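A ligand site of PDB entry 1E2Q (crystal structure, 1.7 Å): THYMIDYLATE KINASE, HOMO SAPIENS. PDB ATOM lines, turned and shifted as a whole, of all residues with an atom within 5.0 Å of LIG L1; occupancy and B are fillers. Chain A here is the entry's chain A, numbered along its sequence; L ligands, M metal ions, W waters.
An oxygen (O3) of LG2 L2 sits close to an oxygen (O1) of LIG L1 (2.5 Å).
Water W6 lies within hydrogen-bond range of the backbone carbonyl oxygen of Arg 153 (2.5 Å) and an oxygen (O6) of LIG L1 (2.7 Å). Water W4 lies within hydrogen-bond range of O7 of LIG L1 and OH of Tyr 154. Water W1 bridges OD1 of Asp 99 (2.6 Å) and O2 of LIG L1 (2.9 Å). Water W5 bridges N2 of LIG L1 (2.9 Å) and O of Gly 105 (3.0 Å). Water W7 lies within hydrogen-bond range of the backbone carbonyl oxygen of Asp 99 (3.0 Å), the backbone carbonyl oxygen of Phe 45 (3.0 Å) and an oxygen (O2) of LIG L1 (3.1 Å).
An oxygen (O8) of LIG L1 is in hydrogen-bond range of the guanidinium group (NH1) of Arg 79, at 2.7 Å. The guanidinium group (NE) of Arg 100 lies within salt-bridge range of an oxygen (O2) of LIG L1. The side-chain carboxylate of Asp 18 lies within hydrogen-bond range of an oxygen (O6) of LIG L1 (3.0 Å). An oxygen (O8) of LIG L1 sits close to the backbone NH of Gly 105. NH2 of Arg 48 lies within salt-bridge range of O3 of LIG L1, at 3.9 Å. An oxygen (O2) of LG2 L2 is in salt-bridge range of the guanidinium group (NH2) of Arg 100, 2.9 Å away. OD1 of Asp 18 sits close to O2 of LG2 L2 (3.0 Å). An oxygen (O5) of LG2 L2 sits at hydrogen-bond distance from the backbone NH (N) of Lys 22 (2.9 Å). The side-chain amino group of Lys 22 lies within salt-bridge range of an oxygen (O5) of LG2 L2, 2.9 Å away.
Phe 45 touches LIG L1. Pro 46 touches LIG L1. CD1 of Leu 60 touches O5 of LIG L1, at 3.6 Å. Phe 75 touches LIG L1. Ser 104 touches LIG L1 (CB to C8, 3.9 Å). Phe 108 touches LIG L1. Tyr 154 touches LIG L1. 12 residues have an atom within 4 Å of LIG L1: Asp 18, Phe 45, Pro 46, Arg 48, Leu 60, Phe 75, Arg 79, Arg 100, Ser 104, Gly 105, Phe 108 and Tyr 154. Along chain A the residues within 4 Å of LIG L1 span positions 18 to 154.
NH1 of Arg 79 is in hydrogen-bond range of O of Phe 75. The guanidinium group (NH1) of Arg 100 lies within hydrogen-bond range of the side-chain hydroxyl (OG) of Ser 104. The backbone NH of Phe 45 lies within hydrogen-bond range of the backbone carbonyl oxygen of Asp 99. The backbone NH (N) of Arg 153 lies within hydrogen-bond range of the backbone carbonyl oxygen (O) of Leu 60. NH1 of Arg 48 is in salt-bridge range of OE2 of Glu 152, 3.4 Å away.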
ATOM      1  N   ASP A  18     -18.175  14.383 -20.746  1.00  0.00           N
ATOM      2  CA  ASP A  18     -17.762  14.717 -19.373  1.00  0.00           C
ATOM      3  C   ASP A  18     -17.972  13.501 -18.475  1.00  0.00           C
ATOM      4  O   ASP A  18     -18.867  12.672 -18.600  1.00  0.00           O
ATOM      5  CB  ASP A  18     -18.528  15.986 -18.958  1.00  0.00           C
ATOM      6  CG  ASP A  18     -18.124  17.195 -19.763  1.00  0.00           C
ATOM      7  OD1 ASP A  18     -16.951  17.199 -20.203  1.00  0.00           O
ATOM      8  OD2 ASP A  18     -18.819  18.214 -20.027  1.00  0.00           O
ATOM      9  N   LYS A  22     -11.523  10.393 -18.735  1.00  0.00           N
ATOM     10  CA  LYS A  22     -10.424  10.849 -19.544  1.00  0.00           C
ATOM     11  C   LYS A  22      -9.199  11.315 -18.761  1.00  0.00           C
ATOM     12  O   LYS A  22      -8.063  10.961 -19.045  1.00  0.00           O
ATOM     13  CB  LYS A  22     -10.841  12.047 -20.460  1.00  0.00           C
ATOM     14  CG  LYS A  22     -12.070  11.625 -21.293  1.00  0.00           C
ATOM     15  CD  LYS A  22     -12.414  12.732 -22.291  1.00  0.00           C
ATOM     16  CE  LYS A  22     -12.828  14.012 -21.565  1.00  0.00           C
ATOM     17  NZ  LYS A  22     -14.048  13.770 -20.748  1.00  0.00           N
ATOM     18  N   PHE A  45      -6.377  19.644 -23.129  1.00  0.00           N
ATOM     19  CA  PHE A  45      -7.060  20.820 -23.687  1.00  0.00           C
ATOM     20  C   PHE A  45      -8.410  20.916 -23.017  1.00  0.00           C
ATOM     21  O   PHE A  45      -9.136  19.957 -22.788  1.00  0.00           O
ATOM     22  CB  PHE A  45      -7.123  20.695 -25.215  1.00  0.00           C
ATOM     23  CG  PHE A  45      -5.757  20.797 -25.820  1.00  0.00           C
ATOM     24  CD1 PHE A  45      -5.157  22.061 -25.895  1.00  0.00           C
ATOM     25  CD2 PHE A  45      -5.078  19.685 -26.282  1.00  0.00           C
ATOM     26  CE1 PHE A  45      -3.869  22.172 -26.411  1.00  0.00           C
ATOM     27  CE2 PHE A  45      -3.792  19.820 -26.802  1.00  0.00           C
ATOM     28  CZ  PHE A  45      -3.188  21.066 -26.885  1.00  0.00           C
ATOM     29  N   PRO A  46      -8.879  22.165 -22.723  1.00  0.00           N
ATOM     30  CA  PRO A  46      -8.052  23.331 -22.910  1.00  0.00           C
ATOM     31  C   PRO A  46      -6.857  23.412 -21.984  1.00  0.00           C
ATOM     32  O   PRO A  46      -6.867  22.830 -20.844  1.00  0.00           O
ATOM     33  CB  PRO A  46      -9.004  24.494 -22.507  1.00  0.00           C
ATOM     34  CG  PRO A  46      -9.961  23.848 -21.574  1.00  0.00           C
ATOM     35  CD  PRO A  46     -10.168  22.419 -22.072  1.00  0.00           C
ATOM     36  N   ARG A  48      -5.345  25.627 -19.773  1.00  0.00           N
ATOM     37  CA  ARG A  48      -5.821  26.872 -19.151  1.00  0.00           C
ATOM     38  C   ARG A  48      -4.743  27.796 -18.664  1.00  0.00           C
ATOM     39  O   ARG A  48      -5.109  28.857 -18.124  1.00  0.00           O
ATOM     40  CB  ARG A  48      -6.755  26.472 -18.002  1.00  0.00           C
ATOM     41  CG  ARG A  48      -7.935  25.590 -18.411  1.00  0.00           C
ATOM     42  CD  ARG A  48      -8.812  25.308 -17.198  1.00  0.00           C
ATOM     43  NE  ARG A  48      -9.897  24.388 -17.470  1.00  0.00           N
ATOM     44  CZ  ARG A  48     -11.123  24.526 -16.977  1.00  0.00           C
ATOM     45  NH1 ARG A  48     -11.500  25.517 -16.187  1.00  0.00           N
ATOM     46  NH2 ARG A  48     -12.000  23.588 -17.326  1.00  0.00           N
ATOM     47  N   LEU A  60     -15.863  28.686 -19.056  1.00  0.00           N
ATOM     48  CA  LEU A  60     -16.372  27.397 -18.579  1.00  0.00           C
ATOM     49  C   LEU A  60     -16.930  27.480 -17.158  1.00  0.00           C
ATOM     50  O   LEU A  60     -17.832  26.720 -16.818  1.00  0.00           O
ATOM     51  CB  LEU A  60     -15.222  26.357 -18.677  1.00  0.00           C
ATOM     52  CG  LEU A  60     -14.995  25.883 -20.123  1.00  0.00           C
ATOM     53  CD1 LEU A  60     -13.745  25.010 -20.192  1.00  0.00           C
ATOM     54  CD2 LEU A  60     -16.238  25.223 -20.709  1.00  0.00           C
ATOM     55  N   PHE A  75     -10.951  28.064 -28.441  1.00  0.00           N
ATOM     56  CA  PHE A  75     -10.551  26.670 -28.096  1.00  0.00           C
ATOM     57  C   PHE A  75      -9.567  26.117 -29.118  1.00  0.00           C
ATOM     58  O   PHE A  75      -8.589  25.451 -28.815  1.00  0.00           O
ATOM     59  CB  PHE A  75     -11.800  25.775 -28.038  1.00  0.00           C
ATOM     60  CG  PHE A  75     -12.487  25.706 -26.698  1.00  0.00           C
ATOM     61  CD1 PHE A  75     -11.844  25.111 -25.607  1.00  0.00           C
ATOM     62  CD2 PHE A  75     -13.757  26.240 -26.534  1.00  0.00           C
ATOM     63  CE1 PHE A  75     -12.485  25.052 -24.391  1.00  0.00           C
ATOM     64  CE2 PHE A  75     -14.398  26.166 -25.310  1.00  0.00           C
ATOM     65  CZ  PHE A  75     -13.780  25.557 -24.228  1.00  0.00           C
ATOM     66  N   ARG A  79      -5.269  25.119 -29.069  1.00  0.00           N
ATOM     67  CA  ARG A  79      -4.525  23.940 -29.547  1.00  0.00           C
ATOM     68  C   ARG A  79      -3.378  24.401 -30.418  1.00  0.00           C
ATOM     69  O   ARG A  79      -2.239  23.956 -30.248  1.00  0.00           O
ATOM     70  CB  ARG A  79      -5.423  22.942 -30.298  1.00  0.00           C
ATOM     71  CG  ARG A  79      -6.306  22.168 -29.314  1.00  0.00           C
ATOM     72  CD  ARG A  79      -7.275  21.321 -30.113  1.00  0.00           C
ATOM     73  NE  ARG A  79      -8.410  21.961 -30.741  1.00  0.00           N
ATOM     74  CZ  ARG A  79      -9.517  22.315 -30.090  1.00  0.00           C
ATOM     75  NH1 ARG A  79      -9.652  22.164 -28.751  1.00  0.00           N
ATOM     76  NH2 ARG A  79     -10.555  22.795 -30.759  1.00  0.00           N
ATOM     77  N   ASP A  99      -5.369  14.746 -23.129  1.00  0.00           N
ATOM     78  CA  ASP A  99      -6.684  14.685 -22.514  1.00  0.00           C
ATOM     79  C   ASP A  99      -7.590  15.727 -23.165  1.00  0.00           C
ATOM     80  O   ASP A  99      -7.468  16.898 -22.786  1.00  0.00           O
ATOM     81  CB  ASP A  99      -6.437  14.952 -21.029  1.00  0.00           C
ATOM     82  CG  ASP A  99      -7.661  14.909 -20.156  1.00  0.00           C
ATOM     83  OD1 ASP A  99      -8.815  14.660 -20.613  1.00  0.00           O
ATOM     84  OD2 ASP A  99      -7.464  15.239 -18.939  1.00  0.00           O
ATOM     85  N   ARG A 100      -8.361  15.292 -24.128  1.00  0.00           N
ATOM     86  CA  ARG A 100      -9.236  16.041 -25.010  1.00  0.00           C
ATOM     87  C   ARG A 100      -8.414  16.740 -26.108  1.00  0.00           C
ATOM     88  O   ARG A 100      -7.248  17.135 -25.896  1.00  0.00           O
ATOM     89  CB  ARG A 100     -10.125  17.097 -24.334  1.00  0.00           C
ATOM     90  CG  ARG A 100     -11.113  16.493 -23.313  1.00  0.00           C
ATOM     91  CD  ARG A 100     -12.020  17.669 -22.889  1.00  0.00           C
ATOM     92  NE  ARG A 100     -13.133  17.322 -22.054  1.00  0.00           N
ATOM     93  CZ  ARG A 100     -14.314  16.769 -22.297  1.00  0.00           C
ATOM     94  NH1 ARG A 100     -14.752  16.359 -23.489  1.00  0.00           N
ATOM     95  NH2 ARG A 100     -15.023  16.626 -21.154  1.00  0.00           N
ATOM     96  N   TYR A 101      -9.017  16.824 -27.314  1.00  0.00           N
ATOM     97  CA  TYR A 101      -8.322  17.493 -28.412  1.00  0.00           C
ATOM     98  C   TYR A 101      -9.363  18.126 -29.323  1.00  0.00           C
ATOM     99  O   TYR A 101     -10.428  18.540 -28.859  1.00  0.00           O
ATOM    100  CB  TYR A 101      -7.487  16.462 -29.170  1.00  0.00           C
ATOM    101  CG  TYR A 101      -6.395  16.896 -30.109  1.00  0.00           C
ATOM    102  CD1 TYR A 101      -5.410  17.807 -29.695  1.00  0.00           C
ATOM    103  CD2 TYR A 101      -6.316  16.387 -31.408  1.00  0.00           C
ATOM    104  CE1 TYR A 101      -4.385  18.145 -30.555  1.00  0.00           C
ATOM    105  CE2 TYR A 101      -5.270  16.731 -32.269  1.00  0.00           C
ATOM    106  CZ  TYR A 101      -4.321  17.613 -31.835  1.00  0.00           C
ATOM    107  OH  TYR A 101      -3.273  17.982 -32.653  1.00  0.00           O
ATOM    108  N   SER A 104     -13.326  17.037 -29.067  1.00  0.00           N
ATOM    109  CA  SER A 104     -14.158  17.678 -28.037  1.00  0.00           C
ATOM    110  C   SER A 104     -14.576  19.067 -28.578  1.00  0.00           C
ATOM    111  O   SER A 104     -15.697  19.521 -28.409  1.00  0.00           O
ATOM    112  CB  SER A 104     -13.423  17.878 -26.719  1.00  0.00           C
ATOM    113  OG  SER A 104     -13.462  16.691 -25.895  1.00  0.00           O
ATOM    114  N   GLY A 105     -13.630  19.732 -29.211  1.00  0.00           N
ATOM    115  CA  GLY A 105     -13.929  21.117 -29.730  1.00  0.00           C
ATOM    116  C   GLY A 105     -15.159  21.053 -30.637  1.00  0.00           C
ATOM    117  O   GLY A 105     -16.056  21.912 -30.577  1.00  0.00           O
ATOM    118  N   PHE A 108     -18.643  19.703 -28.747  1.00  0.00           N
ATOM    119  CA  PHE A 108     -19.293  20.611 -27.842  1.00  0.00           C
ATOM    120  C   PHE A 108     -19.888  21.806 -28.594  1.00  0.00           C
ATOM    121  O   PHE A 108     -21.063  22.105 -28.332  1.00  0.00           O
ATOM    122  CB  PHE A 108     -18.337  20.988 -26.703  1.00  0.00           C
ATOM    123  CG  PHE A 108     -18.379  19.814 -25.732  1.00  0.00           C
ATOM    124  CD1 PHE A 108     -17.621  18.678 -25.950  1.00  0.00           C
ATOM    125  CD2 PHE A 108     -19.223  19.863 -24.640  1.00  0.00           C
ATOM    126  CE1 PHE A 108     -17.674  17.610 -25.072  1.00  0.00           C
ATOM    127  CE2 PHE A 108     -19.290  18.793 -23.764  1.00  0.00           C
ATOM    128  CZ  PHE A 108     -18.524  17.662 -23.988  1.00  0.00           C
ATOM    129  N   GLU A 152     -20.127  23.787 -13.797  1.00  0.00           N
ATOM    130  CA  GLU A 152     -19.478  24.338 -14.981  1.00  0.00           C
ATOM    131  C   GLU A 152     -20.412  24.256 -16.190  1.00  0.00           C
ATOM    132  O   GLU A 152     -21.355  23.487 -16.301  1.00  0.00           O
ATOM    133  CB  GLU A 152     -18.117  23.693 -15.297  1.00  0.00           C
ATOM    134  CG  GLU A 152     -16.887  24.280 -14.630  1.00  0.00           C
ATOM    135  CD  GLU A 152     -15.571  24.101 -15.360  1.00  0.00           C
ATOM    136  OE1 GLU A 152     -15.445  23.254 -16.278  1.00  0.00           O
ATOM    137  OE2 GLU A 152     -14.586  24.807 -15.013  1.00  0.00           O
ATOM    138  N   ARG A 153     -20.150  25.127 -17.168  1.00  0.00           N
ATOM    139  CA  ARG A 153     -20.891  25.175 -18.416  1.00  0.00           C
ATOM    140  C   ARG A 153     -20.995  23.791 -19.061  1.00  0.00           C
ATOM    141  O   ARG A 153     -20.055  23.002 -18.956  1.00  0.00           O
ATOM    142  CB  ARG A 153     -20.068  26.104 -19.326  1.00  0.00           C
ATOM    143  CG  ARG A 153     -20.588  26.355 -20.709  1.00  0.00           C
ATOM    144  CD  ARG A 153     -21.293  27.689 -20.831  1.00  0.00           C
ATOM    145  NE  ARG A 153     -20.493  28.836 -20.391  1.00  0.00           N
ATOM    146  CZ  ARG A 153     -21.072  30.019 -20.159  1.00  0.00           C
ATOM    147  NH1 ARG A 153     -22.388  30.131 -20.329  1.00  0.00           N
ATOM    148  NH2 ARG A 153     -20.411  31.091 -19.773  1.00  0.00           N
ATOM    149  N   TYR A 154     -22.100  23.476 -19.717  1.00  0.00           N
ATOM    150  CA  TYR A 154     -22.327  22.246 -20.446  1.00  0.00           C
ATOM    151  C   TYR A 154     -22.645  21.055 -19.535  1.00  0.00           C
ATOM    152  O   TYR A 154     -22.933  19.962 -20.024  1.00  0.00           O
ATOM    153  CB  TYR A 154     -21.174  21.845 -21.367  1.00  0.00           C
ATOM    154  CG  TYR A 154     -20.715  22.894 -22.361  1.00  0.00           C
ATOM    155  CD1 TYR A 154     -21.628  23.799 -22.912  1.00  0.00           C
ATOM    156  CD2 TYR A 154     -19.389  22.982 -22.756  1.00  0.00           C
ATOM    157  CE1 TYR A 154     -21.194  24.773 -23.802  1.00  0.00           C
ATOM    158  CE2 TYR A 154     -18.963  23.927 -23.661  1.00  0.00           C
ATOM    159  CZ  TYR A 154     -19.877  24.836 -24.171  1.00  0.00           C
ATOM    160  OH  TYR A 154     -19.415  25.775 -25.067  1.00  0.00           O
HETATM  161  P1  LIG L   1     -12.851  18.995 -19.187  1.00  0.00           P
HETATM  162  O1  LIG L   1     -14.065  18.141 -18.899  1.00  0.00           O
HETATM  163  O2  LIG L   1     -11.729  18.384 -19.904  1.00  0.00           O
HETATM  164  O3  LIG L   1     -12.508  19.752 -17.817  1.00  0.00           O
HETATM  165  O4  LIG L   1     -13.328  20.193 -20.134  1.00  0.00           O
HETATM  166  C1  LIG L   1     -14.105  21.351 -19.726  1.00  0.00           C
HETATM  167  C2  LIG L   1     -15.016  21.588 -20.961  1.00  0.00           C
HETATM  168  O5  LIG L   1     -14.536  22.133 -22.170  1.00  0.00           O
HETATM  169  C3  LIG L   1     -15.763  20.304 -21.269  1.00  0.00           C
HETATM  170  O6  LIG L   1     -17.169  20.490 -21.077  1.00  0.00           O
HETATM  171  C4  LIG L   1     -15.484  20.089 -22.766  1.00  0.00           C
HETATM  172  C5  LIG L   1     -15.159  21.509 -23.259  1.00  0.00           C
HETATM  173  N1  LIG L   1     -14.386  21.751 -24.464  1.00  0.00           N
HETATM  174  C6  LIG L   1     -14.972  22.551 -25.482  1.00  0.00           C
HETATM  175  O7  LIG L   1     -16.122  22.993 -25.450  1.00  0.00           O
HETATM  176  N2  LIG L   1     -14.151  22.721 -26.550  1.00  0.00           N
HETATM  177  C7  LIG L   1     -12.857  22.239 -26.616  1.00  0.00           C
HETATM  178  O8  LIG L   1     -12.111  22.491 -27.733  1.00  0.00           O
HETATM  179  C8  LIG L   1     -12.292  21.447 -25.502  1.00  0.00           C
HETATM  180  C9  LIG L   1     -10.888  20.922 -25.613  1.00  0.00           C
HETATM  181  C10 LIG L   1     -13.138  21.264 -24.443  1.00  0.00           C
HETATM  182  P1  LG2 L   2     -14.320  15.833 -17.291  1.00  0.00           P
HETATM  183  O1  LG2 L   2     -15.154  16.610 -16.316  1.00  0.00           O
HETATM  184  O2  LG2 L   2     -15.055  15.517 -18.524  1.00  0.00           O
HETATM  185  O3  LG2 L   2     -12.979  16.498 -17.314  1.00  0.00           O
HETATM  186  P2  LG2 L   2     -13.216  13.123 -17.091  1.00  0.00           P
HETATM  187  O4  LG2 L   2     -11.898  13.766 -17.127  1.00  0.00           O
HETATM  188  O5  LG2 L   2     -13.631  12.357 -18.277  1.00  0.00           O
HETATM  189  O6  LG2 L   2     -14.245  14.326 -16.694  1.00  0.00           O
HETATM  190  P3  LG2 L   2     -12.407  11.941 -14.531  1.00  0.00           P
HETATM  191  O7  LG2 L   2     -11.232  11.115 -14.918  1.00  0.00           O
HETATM  192  O8  LG2 L   2     -12.114  13.216 -13.842  1.00  0.00           O
HETATM  193  O9  LG2 L   2     -13.315  12.156 -15.839  1.00  0.00           O
HETATM  194  O10 LG2 L   2     -13.340  11.081 -13.634  1.00  0.00           O
HETATM  195  C1  LG2 L   2     -14.586  11.672 -13.084  1.00  0.00           C
HETATM  196  C2  LG2 L   2     -14.932  11.000 -11.872  1.00  0.00           C
HETATM  197  O11 LG2 L   2     -15.243   9.618 -12.029  1.00  0.00           O
HETATM  198  C3  LG2 L   2     -13.773  11.072 -10.868  1.00  0.00           C
HETATM  199  O12 LG2 L   2     -14.274  11.195  -9.508  1.00  0.00           O
HETATM  200  C4  LG2 L   2     -13.131   9.703 -10.952  1.00  0.00           C
HETATM  201  O13 LG2 L   2     -12.440   9.157  -9.846  1.00  0.00           O
HETATM  202  C5  LG2 L   2     -14.363   8.792 -11.223  1.00  0.00           C
HETATM  203  N1  LG2 L   2     -13.977   7.722 -12.184  1.00  0.00           N
HETATM  204  C6  LG2 L   2     -13.023   7.769 -13.207  1.00  0.00           C
HETATM  205  N2  LG2 L   2     -13.004   6.578 -13.768  1.00  0.00           N
HETATM  206  C7  LG2 L   2     -13.889   5.748 -13.135  1.00  0.00           C
HETATM  207  C8  LG2 L   2     -14.254   4.403 -13.305  1.00  0.00           C
HETATM  208  N3  LG2 L   2     -13.678   3.632 -14.232  1.00  0.00           N
HETATM  209  N4  LG2 L   2     -15.179   4.031 -12.442  1.00  0.00           N
HETATM  210  C9  LG2 L   2     -15.792   4.788 -11.503  1.00  0.00           C
HETATM  211  N5  LG2 L   2     -15.480   6.064 -11.308  1.00  0.00           N
HETATM  212  C10 LG2 L   2     -14.556   6.440 -12.131  1.00  0.00           C
HETATM  213 MG    MG M   1     -11.127  15.675 -17.076  1.00  0.00          MG
HETATM  214  O   HOH W   1     -10.770  15.778 -19.239  1.00  0.00           O
HETATM  215  O   HOH W   2     -10.268  17.562 -16.827  1.00  0.00           O
HETATM  216  O   HOH W   3     -10.665  20.155 -15.043  1.00  0.00           O
HETATM  217  O   HOH W   4     -17.588  24.755 -26.901  1.00  0.00           O
HETATM  218  O   HOH W   5     -15.063  24.128 -28.867  1.00  0.00           O
HETATM  219  O   HOH W   6     -17.799  21.857 -18.860  1.00  0.00           O
HETATM  220  O   HOH W   7      -8.718  18.173 -20.416  1.00  0.00           O
